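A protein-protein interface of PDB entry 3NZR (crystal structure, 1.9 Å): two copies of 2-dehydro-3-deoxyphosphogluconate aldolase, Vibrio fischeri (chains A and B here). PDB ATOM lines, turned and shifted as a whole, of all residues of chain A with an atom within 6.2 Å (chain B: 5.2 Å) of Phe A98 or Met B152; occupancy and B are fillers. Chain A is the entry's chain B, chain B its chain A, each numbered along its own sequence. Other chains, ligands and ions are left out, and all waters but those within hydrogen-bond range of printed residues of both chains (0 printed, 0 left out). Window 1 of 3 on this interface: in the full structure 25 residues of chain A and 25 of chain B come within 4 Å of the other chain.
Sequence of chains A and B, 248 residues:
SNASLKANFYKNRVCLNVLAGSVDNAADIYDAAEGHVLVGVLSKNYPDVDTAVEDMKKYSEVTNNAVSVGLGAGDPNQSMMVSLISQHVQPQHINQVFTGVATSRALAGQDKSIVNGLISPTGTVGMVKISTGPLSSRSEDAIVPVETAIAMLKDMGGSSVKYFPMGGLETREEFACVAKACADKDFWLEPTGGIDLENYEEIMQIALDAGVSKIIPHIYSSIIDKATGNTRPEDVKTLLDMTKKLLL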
ATOM      1  N   GLN A  96       4.230 -18.428  15.046  1.00  0.00           N
ATOM      2  CA  GLN A  96       3.944 -19.798  15.215  1.00  0.00           C
ATOM      3  C   GLN A  96       4.296 -20.597  13.987  1.00  0.00           C
ATOM      4  O   GLN A  96       4.597 -20.028  12.941  1.00  0.00           O
ATOM      5  CB  GLN A  96       2.448 -20.049  15.510  1.00  0.00           C
ATOM      6  CG  GLN A  96       2.145 -20.059  16.983  1.00  0.00           C
ATOM      7  CD  GLN A  96       2.894 -21.032  17.753  1.00  0.00           C
ATOM      8  OE1 GLN A  96       3.386 -22.051  17.201  1.00  0.00           O
ATOM      9  NE2 GLN A  96       2.923 -20.832  19.109  1.00  0.00           N
ATOM     10  N   VAL A  97       4.289 -21.935  14.180  1.00  0.00           N
ATOM     11  CA  VAL A  97       4.407 -22.859  13.148  1.00  0.00           C
ATOM     12  C   VAL A  97       2.973 -23.221  12.771  1.00  0.00           C
ATOM     13  O   VAL A  97       2.053 -22.851  13.504  1.00  0.00           O
ATOM     14  CB  VAL A  97       5.223 -24.085  13.537  1.00  0.00           C
ATOM     15  CG1 VAL A  97       6.674 -23.602  13.838  1.00  0.00           C
ATOM     16  CG2 VAL A  97       4.585 -24.836  14.694  1.00  0.00           C
ATOM     17  N   PHE A  98       2.778 -23.909  11.663  1.00  0.00           N
ATOM     18  CA  PHE A  98       1.446 -24.078  11.089  1.00  0.00           C
ATOM     19  C   PHE A  98       0.536 -24.775  12.084  1.00  0.00           C
ATOM     20  O   PHE A  98      -0.617 -24.375  12.228  1.00  0.00           O
ATOM     21  CB  PHE A  98       1.527 -24.889   9.794  1.00  0.00           C
ATOM     22  CG  PHE A  98       0.241 -24.972   9.054  1.00  0.00           C
ATOM     23  CD1 PHE A  98      -0.099 -24.006   8.154  1.00  0.00           C
ATOM     24  CD2 PHE A  98      -0.608 -26.086   9.230  1.00  0.00           C
ATOM     25  CE1 PHE A  98      -1.306 -24.116   7.430  1.00  0.00           C
ATOM     26  CE2 PHE A  98      -1.804 -26.194   8.486  1.00  0.00           C
ATOM     27  CZ  PHE A  98      -2.120 -25.219   7.589  1.00  0.00           C
ATOM     28  N   THR A  99       1.053 -25.726  12.809  1.00  0.00           N
ATOM     29  CA  THR A  99       0.249 -26.497  13.744  1.00  0.00           C
ATOM     30  C   THR A  99      -0.003 -25.837  15.096  1.00  0.00           C
ATOM     31  O   THR A  99      -0.554 -26.478  16.043  1.00  0.00           O
ATOM     32  CB  THR A  99       0.952 -27.816  13.961  1.00  0.00           C
ATOM     33  OG1 THR A  99       2.291 -27.602  14.414  1.00  0.00           O
ATOM     34  CG2 THR A  99       0.965 -28.682  12.651  1.00  0.00           C
ATOM     35  N   GLY A 100       0.516 -24.629  15.276  1.00  0.00           N
ATOM     36  CA  GLY A 100       0.442 -23.928  16.536  1.00  0.00           C
ATOM     37  C   GLY A 100      -0.387 -22.671  16.464  1.00  0.00           C
ATOM     38  O   GLY A 100      -0.588 -21.992  17.535  1.00  0.00           O
ATOM     39  N   VAL A 101      -0.897 -22.365  15.261  1.00  0.00           N
ATOM     40  CA  VAL A 101      -1.642 -21.067  15.007  1.00  0.00           C
ATOM     41  C   VAL A 101      -2.921 -21.047  15.851  1.00  0.00           C
ATOM     42  O   VAL A 101      -3.154 -20.121  16.627  1.00  0.00           O
ATOM     43  CB  VAL A 101      -1.948 -20.850  13.496  1.00  0.00           C
ATOM     44  CG1 VAL A 101      -2.804 -19.575  13.291  1.00  0.00           C
ATOM     45  CG2 VAL A 101      -0.667 -20.575  12.708  1.00  0.00           C
ATOM     46  N   ALA A 102      -3.705 -22.106  15.751  1.00  0.00           N
ATOM     47  CA  ALA A 102      -4.953 -22.214  16.494  1.00  0.00           C
ATOM     48  C   ALA A 102      -4.775 -22.215  17.983  1.00  0.00           C
ATOM     49  O   ALA A 102      -5.580 -21.616  18.703  1.00  0.00           O
ATOM     50  CB  ALA A 102      -5.767 -23.426  16.043  1.00  0.00           C
ATOM     51  N   GLY A 117       1.808 -17.651  10.780  1.00  0.00           N
ATOM     52  CA  GLY A 117       1.964 -19.070  10.617  1.00  0.00           C
ATOM     53  C   GLY A 117       3.016 -19.393   9.579  1.00  0.00           C
ATOM     54  O   GLY A 117       2.930 -19.000   8.396  1.00  0.00           O
ATOM     55  N   LEU A 118       3.943 -20.204  10.004  1.00  0.00           N
ATOM     56  CA  LEU A 118       5.094 -20.635   9.172  1.00  0.00           C
ATOM     57  C   LEU A 118       4.691 -21.572   8.079  1.00  0.00           C
ATOM     58  O   LEU A 118       4.230 -22.677   8.295  1.00  0.00           O
ATOM     59  CB  LEU A 118       6.118 -21.337  10.006  1.00  0.00           C
ATOM     60  CG  LEU A 118       7.500 -21.752   9.390  1.00  0.00           C
ATOM     61  CD1 LEU A 118       8.000 -20.950   8.413  1.00  0.00           C
ATOM     62  CD2 LEU A 118       8.586 -21.891  10.504  1.00  0.00           C
ATOM     63  N   ILE A 119       4.898 -21.131   6.869  1.00  0.00           N
ATOM     64  CA  ILE A 119       4.844 -22.005   5.715  1.00  0.00           C
ATOM     65  C   ILE A 119       6.057 -21.704   4.820  1.00  0.00           C
ATOM     66  O   ILE A 119       6.631 -20.628   4.892  1.00  0.00           O
ATOM     67  CB  ILE A 119       3.525 -21.859   4.919  1.00  0.00           C
ATOM     68  CG1 ILE A 119       3.515 -20.516   4.159  1.00  0.00           C
ATOM     69  CG2 ILE A 119       2.266 -22.052   5.812  1.00  0.00           C
ATOM     70  CD1 ILE A 119       2.282 -20.245   3.298  1.00  0.00           C
ATOM     71  N   ILE A 130       3.447 -26.963   4.433  1.00  0.00           N
ATOM     72  CA  ILE A 130       2.721 -26.595   5.650  1.00  0.00           C
ATOM     73  C   ILE A 130       3.011 -27.538   6.838  1.00  0.00           C
ATOM     74  O   ILE A 130       2.538 -27.307   7.951  1.00  0.00           O
ATOM     75  CB  ILE A 130       1.182 -26.557   5.451  1.00  0.00           C
ATOM     76  CG1 ILE A 130       0.634 -27.898   5.094  1.00  0.00           C
ATOM     77  CG2 ILE A 130       0.720 -25.465   4.489  1.00  0.00           C
ATOM     78  CD1 ILE A 130      -0.864 -27.852   5.118  1.00  0.00           C
ATOM     79  N   SER A 131       3.763 -28.619   6.612  1.00  0.00           N
ATOM     80  CA  SER A 131       4.145 -29.503   7.668  1.00  0.00           C
ATOM     81  C   SER A 131       5.340 -28.948   8.495  1.00  0.00           C
ATOM     82  O   SER A 131       6.392 -29.530   8.465  1.00  0.00           O
ATOM     83  CB  SER A 131       4.535 -30.859   7.061  1.00  0.00           C
ATOM     84  OG  SER A 131       5.263 -30.660   5.843  1.00  0.00           O
ATOM     85  N   THR A 132       5.107 -27.896   9.278  1.00  0.00           N
ATOM     86  CA  THR A 132       6.158 -27.158   9.916  1.00  0.00           C
ATOM     87  C   THR A 132       6.186 -27.304  11.460  1.00  0.00           C
ATOM     88  O   THR A 132       6.947 -26.577  12.178  1.00  0.00           O
ATOM     89  CB  THR A 132       6.098 -25.677   9.524  1.00  0.00           C
ATOM     90  OG1 THR A 132       4.814 -25.120   9.868  1.00  0.00           O
ATOM     91  CG2 THR A 132       6.305 -25.500   8.010  1.00  0.00           C
ATOM     92  N   GLY A 133       5.332 -28.187  11.973  1.00  0.00           N
ATOM     93  CA  GLY A 133       5.223 -28.456  13.393  1.00  0.00           C
ATOM     94  C   GLY A 133       6.257 -29.434  13.960  1.00  0.00           C
ATOM     95  O   GLY A 133       7.052 -30.038  13.221  1.00  0.00           O
ATOM     96  N   LEU A 135       6.445 -32.651  15.203  1.00  0.00           N
ATOM     97  CA  LEU A 135       6.578 -33.944  14.555  1.00  0.00           C
ATOM     98  C   LEU A 135       6.386 -33.842  13.072  1.00  0.00           C
ATOM     99  O   LEU A 135       6.995 -34.601  12.321  1.00  0.00           O
ATOM    100  CB  LEU A 135       5.548 -34.961  15.082  1.00  0.00           C
ATOM    101  CG  LEU A 135       5.681 -35.507  16.501  1.00  0.00           C
ATOM    102  CD1 LEU A 135       4.484 -36.395  16.825  1.00  0.00           C
ATOM    103  CD2 LEU A 135       7.048 -36.287  16.682  1.00  0.00           C
ATOM    104  N   SER A 136       5.514 -32.954  12.612  1.00  0.00           N
ATOM    105  CA  SER A 136       5.256 -32.952  11.183  1.00  0.00           C
ATOM    106  C   SER A 136       6.435 -32.426  10.397  1.00  0.00           C
ATOM    107  O   SER A 136       6.584 -32.850   9.258  1.00  0.00           O
ATOM    108  CB  SER A 136       3.992 -32.193  10.833  1.00  0.00           C
ATOM    109  OG  SER A 136       3.985 -30.885  11.339  1.00  0.00           O
ATOM    110  N   SER A 139       8.334 -35.419   9.111  1.00  0.00           N
ATOM    111  CA  SER A 139       7.719 -36.364   8.185  1.00  0.00           C
ATOM    112  C   SER A 139       7.900 -35.921   6.743  1.00  0.00           C
ATOM    113  O   SER A 139       8.328 -34.789   6.461  1.00  0.00           O
ATOM    114  CB  SER A 139       6.193 -36.499   8.397  1.00  0.00           C
ATOM    115  OG  SER A 139       5.864 -36.546   9.746  1.00  0.00           O
ATOM    116  N   ALA A 142       4.214 -32.035   3.524  1.00  0.00           N
ATOM    117  CA  ALA A 142       2.861 -31.710   3.200  1.00  0.00           C
ATOM    118  C   ALA A 142       2.885 -30.511   2.281  1.00  0.00           C
ATOM    119  O   ALA A 142       3.120 -29.398   2.735  1.00  0.00           O
ATOM    120  CB  ALA A 142       2.096 -31.331   4.490  1.00  0.00           C
ATOM    121  N   THR A 148      -5.147 -22.540  -0.527  1.00  0.00           N
ATOM    122  CA  THR A 148      -5.724 -23.419   0.476  1.00  0.00           C
ATOM    123  C   THR A 148      -4.972 -23.202   1.851  1.00  0.00           C
ATOM    124  O   THR A 148      -5.596 -23.201   2.905  1.00  0.00           O
ATOM    125  CB  THR A 148      -5.604 -24.825  -0.020  1.00  0.00           C
ATOM    126  OG1 THR A 148      -6.204 -24.832  -1.317  1.00  0.00           O
ATOM    127  CG2 THR A 148      -6.358 -25.832   0.870  1.00  0.00           C
ATOM    128  N   ALA A 149      -3.641 -23.044   1.819  1.00  0.00           N
ATOM    129  CA  ALA A 149      -2.815 -22.853   2.998  1.00  0.00           C
ATOM    130  C   ALA A 149      -3.344 -21.629   3.723  1.00  0.00           C
ATOM    131  O   ALA A 149      -3.525 -21.712   4.919  1.00  0.00           O
ATOM    132  CB  ALA A 149      -1.297 -22.656   2.658  1.00  0.00           C
ATOM    133  N   ILE A 150      -3.608 -20.564   2.990  1.00  0.00           N
ATOM    134  CA  ILE A 150      -4.126 -19.312   3.542  1.00  0.00           C
ATOM    135  C   ILE A 150      -5.543 -19.522   4.117  1.00  0.00           C
ATOM    136  O   ILE A 150      -5.891 -19.011   5.164  1.00  0.00           O
ATOM    137  CB  ILE A 150      -4.121 -18.230   2.534  1.00  0.00           C
ATOM    138  CG1 ILE A 150      -2.657 -17.864   2.131  1.00  0.00           C
ATOM    139  CG2 ILE A 150      -4.804 -17.005   3.091  1.00  0.00           C
ATOM    140  CD1 ILE A 150      -2.556 -16.954   0.909  1.00  0.00           C
ATOM    141  N   MET A 152      -6.733 -22.292   5.265  1.00  0.00           N
ATOM    142  CA  MET A 152      -6.577 -23.081   6.509  1.00  0.00           C
ATOM    143  C   MET A 152      -6.073 -22.211   7.630  1.00  0.00           C
ATOM    144  O   MET A 152      -6.537 -22.328   8.768  1.00  0.00           O
ATOM    145  CB  MET A 152      -5.666 -24.334   6.315  1.00  0.00           C
ATOM    146  CG  MET A 152      -6.239 -25.310   5.342  1.00  0.00           C
ATOM    147  SD  MET A 152      -5.023 -26.761   4.922  1.00  0.00           S
ATOM    148  CE  MET A 152      -5.504 -27.932   6.364  1.00  0.00           C
ATOM    149  N   LEU A 153      -5.112 -21.330   7.347  1.00  0.00           N
ATOM    150  CA  LEU A 153      -4.597 -20.435   8.367  1.00  0.00           C
ATOM    151  C   LEU A 153      -5.692 -19.513   8.847  1.00  0.00           C
ATOM    152  O   LEU A 153      -5.778 -19.309  10.019  1.00  0.00           O
ATOM    153  CB  LEU A 153      -3.402 -19.595   7.838  1.00  0.00           C
ATOM    154  CG  LEU A 153      -2.095 -20.311   7.654  1.00  0.00           C
ATOM    155  CD1 LEU A 153      -1.035 -19.402   6.899  1.00  0.00           C
ATOM    156  CD2 LEU A 153      -1.539 -20.650   8.991  1.00  0.00           C
ATOM    157  N   MET A 156      -7.874 -21.290  11.120  1.00  0.00           N
ATOM    158  CA  MET A 156      -7.288 -21.564  12.431  1.00  0.00           C
ATOM    159  C   MET A 156      -7.056 -20.304  13.253  1.00  0.00           C
ATOM    160  O   MET A 156      -6.408 -20.316  14.300  1.00  0.00           O
ATOM    161  CB  MET A 156      -6.013 -22.404  12.288  1.00  0.00           C
ATOM    162  CG  MET A 156      -6.273 -23.682  11.638  1.00  0.00           C
ATOM    163  SD  MET A 156      -4.760 -24.950  11.458  1.00  0.00           S
ATOM    164  CE  MET A 156      -3.446 -23.694  10.600  1.00  0.00           C
ATOM    165  N   PHE B  98     -10.283 -30.722  10.421  1.00  0.00           N
ATOM    166  CA  PHE B  98      -8.811 -30.626  10.593  1.00  0.00           C
ATOM    167  C   PHE B  98      -8.406 -29.304  11.220  1.00  0.00           C
ATOM    168  O   PHE B  98      -7.566 -29.281  12.103  1.00  0.00           O
ATOM    169  CB  PHE B  98      -8.139 -30.820   9.248  1.00  0.00           C
ATOM    170  CG  PHE B  98      -6.633 -30.973   9.302  1.00  0.00           C
ATOM    171  CD1 PHE B  98      -6.067 -32.233   9.471  1.00  0.00           C
ATOM    172  CD2 PHE B  98      -5.795 -29.862   9.114  1.00  0.00           C
ATOM    173  CE1 PHE B  98      -4.702 -32.378   9.499  1.00  0.00           C
ATOM    174  CE2 PHE B  98      -4.421 -30.015   9.161  1.00  0.00           C
ATOM    175  CZ  PHE B  98      -3.892 -31.295   9.321  1.00  0.00           C
ATOM    176  N   ILE B 130      -6.997 -32.911   3.650  1.00  0.00           N
ATOM    177  CA  ILE B 130      -7.052 -32.315   5.009  1.00  0.00           C
ATOM    178  C   ILE B 130      -7.678 -30.910   5.024  1.00  0.00           C
ATOM    179  O   ILE B 130      -7.756 -30.232   6.129  1.00  0.00           O
ATOM    180  CB  ILE B 130      -5.659 -32.234   5.667  1.00  0.00           C
ATOM    181  CG1 ILE B 130      -4.693 -31.437   4.794  1.00  0.00           C
ATOM    182  CG2 ILE B 130      -5.068 -33.667   5.896  1.00  0.00           C
ATOM    183  CD1 ILE B 130      -3.386 -31.101   5.468  1.00  0.00           C
ATOM    184  N   THR B 148       1.936 -37.783   7.337  1.00  0.00           N
ATOM    185  CA  THR B 148       2.172 -36.406   7.760  1.00  0.00           C
ATOM    186  C   THR B 148       0.907 -35.831   8.312  1.00  0.00           C
ATOM    187  O   THR B 148       0.904 -35.013   9.222  1.00  0.00           O
ATOM    188  CB  THR B 148       2.631 -35.635   6.600  1.00  0.00           C
ATOM    189  OG1 THR B 148       3.747 -36.351   6.082  1.00  0.00           O
ATOM    190  CG2 THR B 148       3.057 -34.266   6.929  1.00  0.00           C
ATOM    191  N   ALA B 149      -0.213 -36.216   7.753  1.00  0.00           N
ATOM    192  CA  ALA B 149      -1.519 -35.779   8.364  1.00  0.00           C
ATOM    193  C   ALA B 149      -1.666 -36.245   9.823  1.00  0.00           C
ATOM    194  O   ALA B 149      -2.151 -35.516  10.651  1.00  0.00           O
ATOM    195  CB  ALA B 149      -2.703 -36.337   7.502  1.00  0.00           C
ATOM    196  N   ILE B 150      -1.279 -37.476  10.116  1.00  0.00           N
ATOM    197  CA  ILE B 150      -1.316 -37.976  11.484  1.00  0.00           C
ATOM    198  C   ILE B 150      -0.308 -37.160  12.378  1.00  0.00           C
ATOM    199  O   ILE B 150      -0.602 -36.793  13.528  1.00  0.00           O
ATOM    200  CB  ILE B 150      -0.973 -39.434  11.510  1.00  0.00           C
ATOM    201  CG1 ILE B 150      -2.126 -40.279  10.931  1.00  0.00           C
ATOM    202  CG2 ILE B 150      -0.667 -39.932  12.907  1.00  0.00           C
ATOM    203  CD1 ILE B 150      -1.695 -41.669  10.632  1.00  0.00           C
ATOM    204  N   ALA B 151       0.874 -36.860  11.835  1.00  0.00           N
ATOM    205  CA  ALA B 151       1.875 -36.118  12.577  1.00  0.00           C
ATOM    206  C   ALA B 151       1.367 -34.718  12.893  1.00  0.00           C
ATOM    207  O   ALA B 151       1.525 -34.224  13.995  1.00  0.00           O
ATOM    208  CB  ALA B 151       3.202 -36.113  11.866  1.00  0.00           C
ATOM    209  N   MET B 152       0.659 -34.127  11.961  1.00  0.00           N
ATOM    210  CA  MET B 152       0.096 -32.779  12.153  1.00  0.00           C
ATOM    211  C   MET B 152      -1.055 -32.823  13.144  1.00  0.00           C
ATOM    212  O   MET B 152      -1.184 -31.965  13.980  1.00  0.00           O
ATOM    213  CB  MET B 152      -0.351 -32.237  10.794  1.00  0.00           C
ATOM    214  CG  MET B 152       0.744 -31.749   9.939  1.00  0.00           C
ATOM    215  SD  MET B 152       0.152 -31.226   8.131  1.00  0.00           S
ATOM    216  CE  MET B 152      -0.341 -29.363   8.604  1.00  0.00           C
ATOM    217  N   LEU B 153      -1.903 -33.840  13.077  1.00  0.00           N
ATOM    218  CA  LEU B 153      -2.938 -33.995  14.044  1.00  0.00           C
ATOM    219  C   LEU B 153      -2.380 -34.126  15.413  1.00  0.00           C
ATOM    220  O   LEU B 153      -2.901 -33.463  16.326  1.00  0.00           O
ATOM    221  CB  LEU B 153      -3.874 -35.183  13.688  1.00  0.00           C
ATOM    222  CG  LEU B 153      -4.819 -34.942  12.522  1.00  0.00           C
ATOM    223  CD1 LEU B 153      -5.496 -36.286  12.090  1.00  0.00           C
ATOM    224  CD2 LEU B 153      -5.910 -33.967  12.915  1.00  0.00           C
ATOM    225  N   LYS B 154      -1.324 -34.938  15.610  1.00  0.00           N
ATOM    226  CA  LYS B 154      -0.677 -35.008  16.910  1.00  0.00           C
ATOM    227  C   LYS B 154      -0.156 -33.675  17.363  1.00  0.00           C
ATOM    228  O   LYS B 154      -0.395 -33.305  18.514  1.00  0.00           O
ATOM    229  CB  LYS B 154       0.499 -35.961  16.964  1.00  0.00           C
ATOM    230  CG  LYS B 154       0.123 -37.440  16.864  1.00  0.00           C
ATOM    231  CD  LYS B 154       1.437 -38.211  16.892  1.00  0.00           C
ATOM    232  CE  LYS B 154       1.233 -39.670  16.872  1.00  0.00           C
ATOM    233  NZ  LYS B 154       2.542 -40.357  16.948  1.00  0.00           N
ATOM    234  N   ASP B 155       0.570 -32.992  16.461  1.00  0.00           N
ATOM    235  CA  ASP B 155       1.055 -31.634  16.738  1.00  0.00           C
ATOM    236  C   ASP B 155      -0.023 -30.693  17.162  1.00  0.00           C
ATOM    237  O   ASP B 155       0.269 -29.720  17.895  1.00  0.00           O
ATOM    238  CB  ASP B 155       1.777 -30.992  15.536  1.00  0.00           C
ATOM    239  CG  ASP B 155       3.138 -31.701  15.165  1.00  0.00           C
ATOM    240  OD1 ASP B 155       3.729 -32.445  16.031  1.00  0.00           O
ATOM    241  OD2 ASP B 155       3.634 -31.424  14.017  1.00  0.00           O
ATOM    242  N   MET B 156      -1.265 -30.909  16.684  1.00  0.00           N
ATOM    243  CA  MET B 156      -2.361 -30.027  16.989  1.00  0.00           C
ATOM    244  C   MET B 156      -3.210 -30.475  18.219  1.00  0.00           C
ATOM    245  O   MET B 156      -4.254 -29.874  18.478  1.00  0.00           O
ATOM    246  CB  MET B 156      -3.215 -29.884  15.747  1.00  0.00           C
ATOM    247  CG  MET B 156      -2.442 -29.138  14.692  1.00  0.00           C
ATOM    248  SD  MET B 156      -3.471 -28.685  13.097  1.00  0.00           S
ATOM    249  CE  MET B 156      -4.592 -30.214  13.098  1.00  0.00           C
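N of Leu A135 lies within hydrogen-bond range of OD1 of Asp B155 (2.8 Å). The side-chain carboxylate (OD2) of Asp B155 lies within hydrogen-bond range of the side-chain hydroxyl (OG) of Ser A136, 2.8 Å away.
The backbone NH of Gly A133 lies within hydrogen-bond range of the side-chain hydroxyl of Ser A136 (3.1 Å). The backbone NH (N) of Phe A98 sits at hydrogen-bond distance from the side-chain hydroxyl (OG1) of Thr A132 (3.0 Å). O of Leu A135 is in hydrogen-bond range of OG of Ser A139 (3.4 Å). The backbone NH (N) of Ile A130 is in hydrogen-bond range of the backbone carbonyl oxygen (O) of Ala A142 (3.0 Å). OG of Ser A131 lies within hydrogen-bond range of N of Ala A142 (2.9 Å).
Phe A98 touches Met B152. Thr A99 touches Asp B155. Thr A99 touches Met B156 (O to CG, 3.5 Å). Gly A133 touches Asp B155 (C to OD2, 3.3 Å). Leu A135 touches Lys B154 (CD1 to CD, 3.5 Å). Ser A136 touches Ala B151. Ser A139 touches Thr B148. Ala A142 touches Thr B148. Met A152 touches Phe B98. Ile B130 touches Met A152.
Of chain B, only Met B152 comes within 4 Å of Phe A98. Of the printed residues of chain B, Gly A133 touches Asp B155 (3.3 Å). Ile A150 touches none of the printed residues of chain B. Of the printed residues of chain B, Met A152 touches Phe B98 and Ile B130. Printed residues of chain A within 4 Å of Phe B98: Met A152 (3.4 Å). Printed residues of chain A within 4 Å of Ile B130: Met A152. Printed residues of chain A within 4 Å of Thr B148: Ser A131, Ser A139 and Ala A142. Ala B149 touches none of the printed residues of chain A. Met B152 touches just these residues of chain A: Phe A98, Ile A130 and Ser A136. The nearest residue of chain B that does not touch Phe A98 is Phe B98 (4.7 Å). The nearest printed residue of chain B that does not touch Thr A99 is Met B152 (4.1 Å).
Hydrophobic or aromatic side chains of chain B that line the printed part of chain A: Phe B98, Ile B130, Ala B151, Met B152 and Met B156. Printed residues of chain A that touch a printed residue of chain B: Phe A98, Thr A99, Ile A130, Ser A131, Gly A133, Leu A135, Ser A136, Ser A139, Ala A142 and Met A152. Hydrophobic or aromatic side chains of chain A within 4 Å of the printed part of chain B: Phe A98, Ile A130, Leu A135, Ala A142 and Met A152. Among the printed residues, 16 pairs touch across the chains.
Phe A98 touches Met B152, and with the chains exchanged Met A152 touches Phe B98. Ile A130 touches Met B152, and with the chains exchanged Met A152 touches Ile B130.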
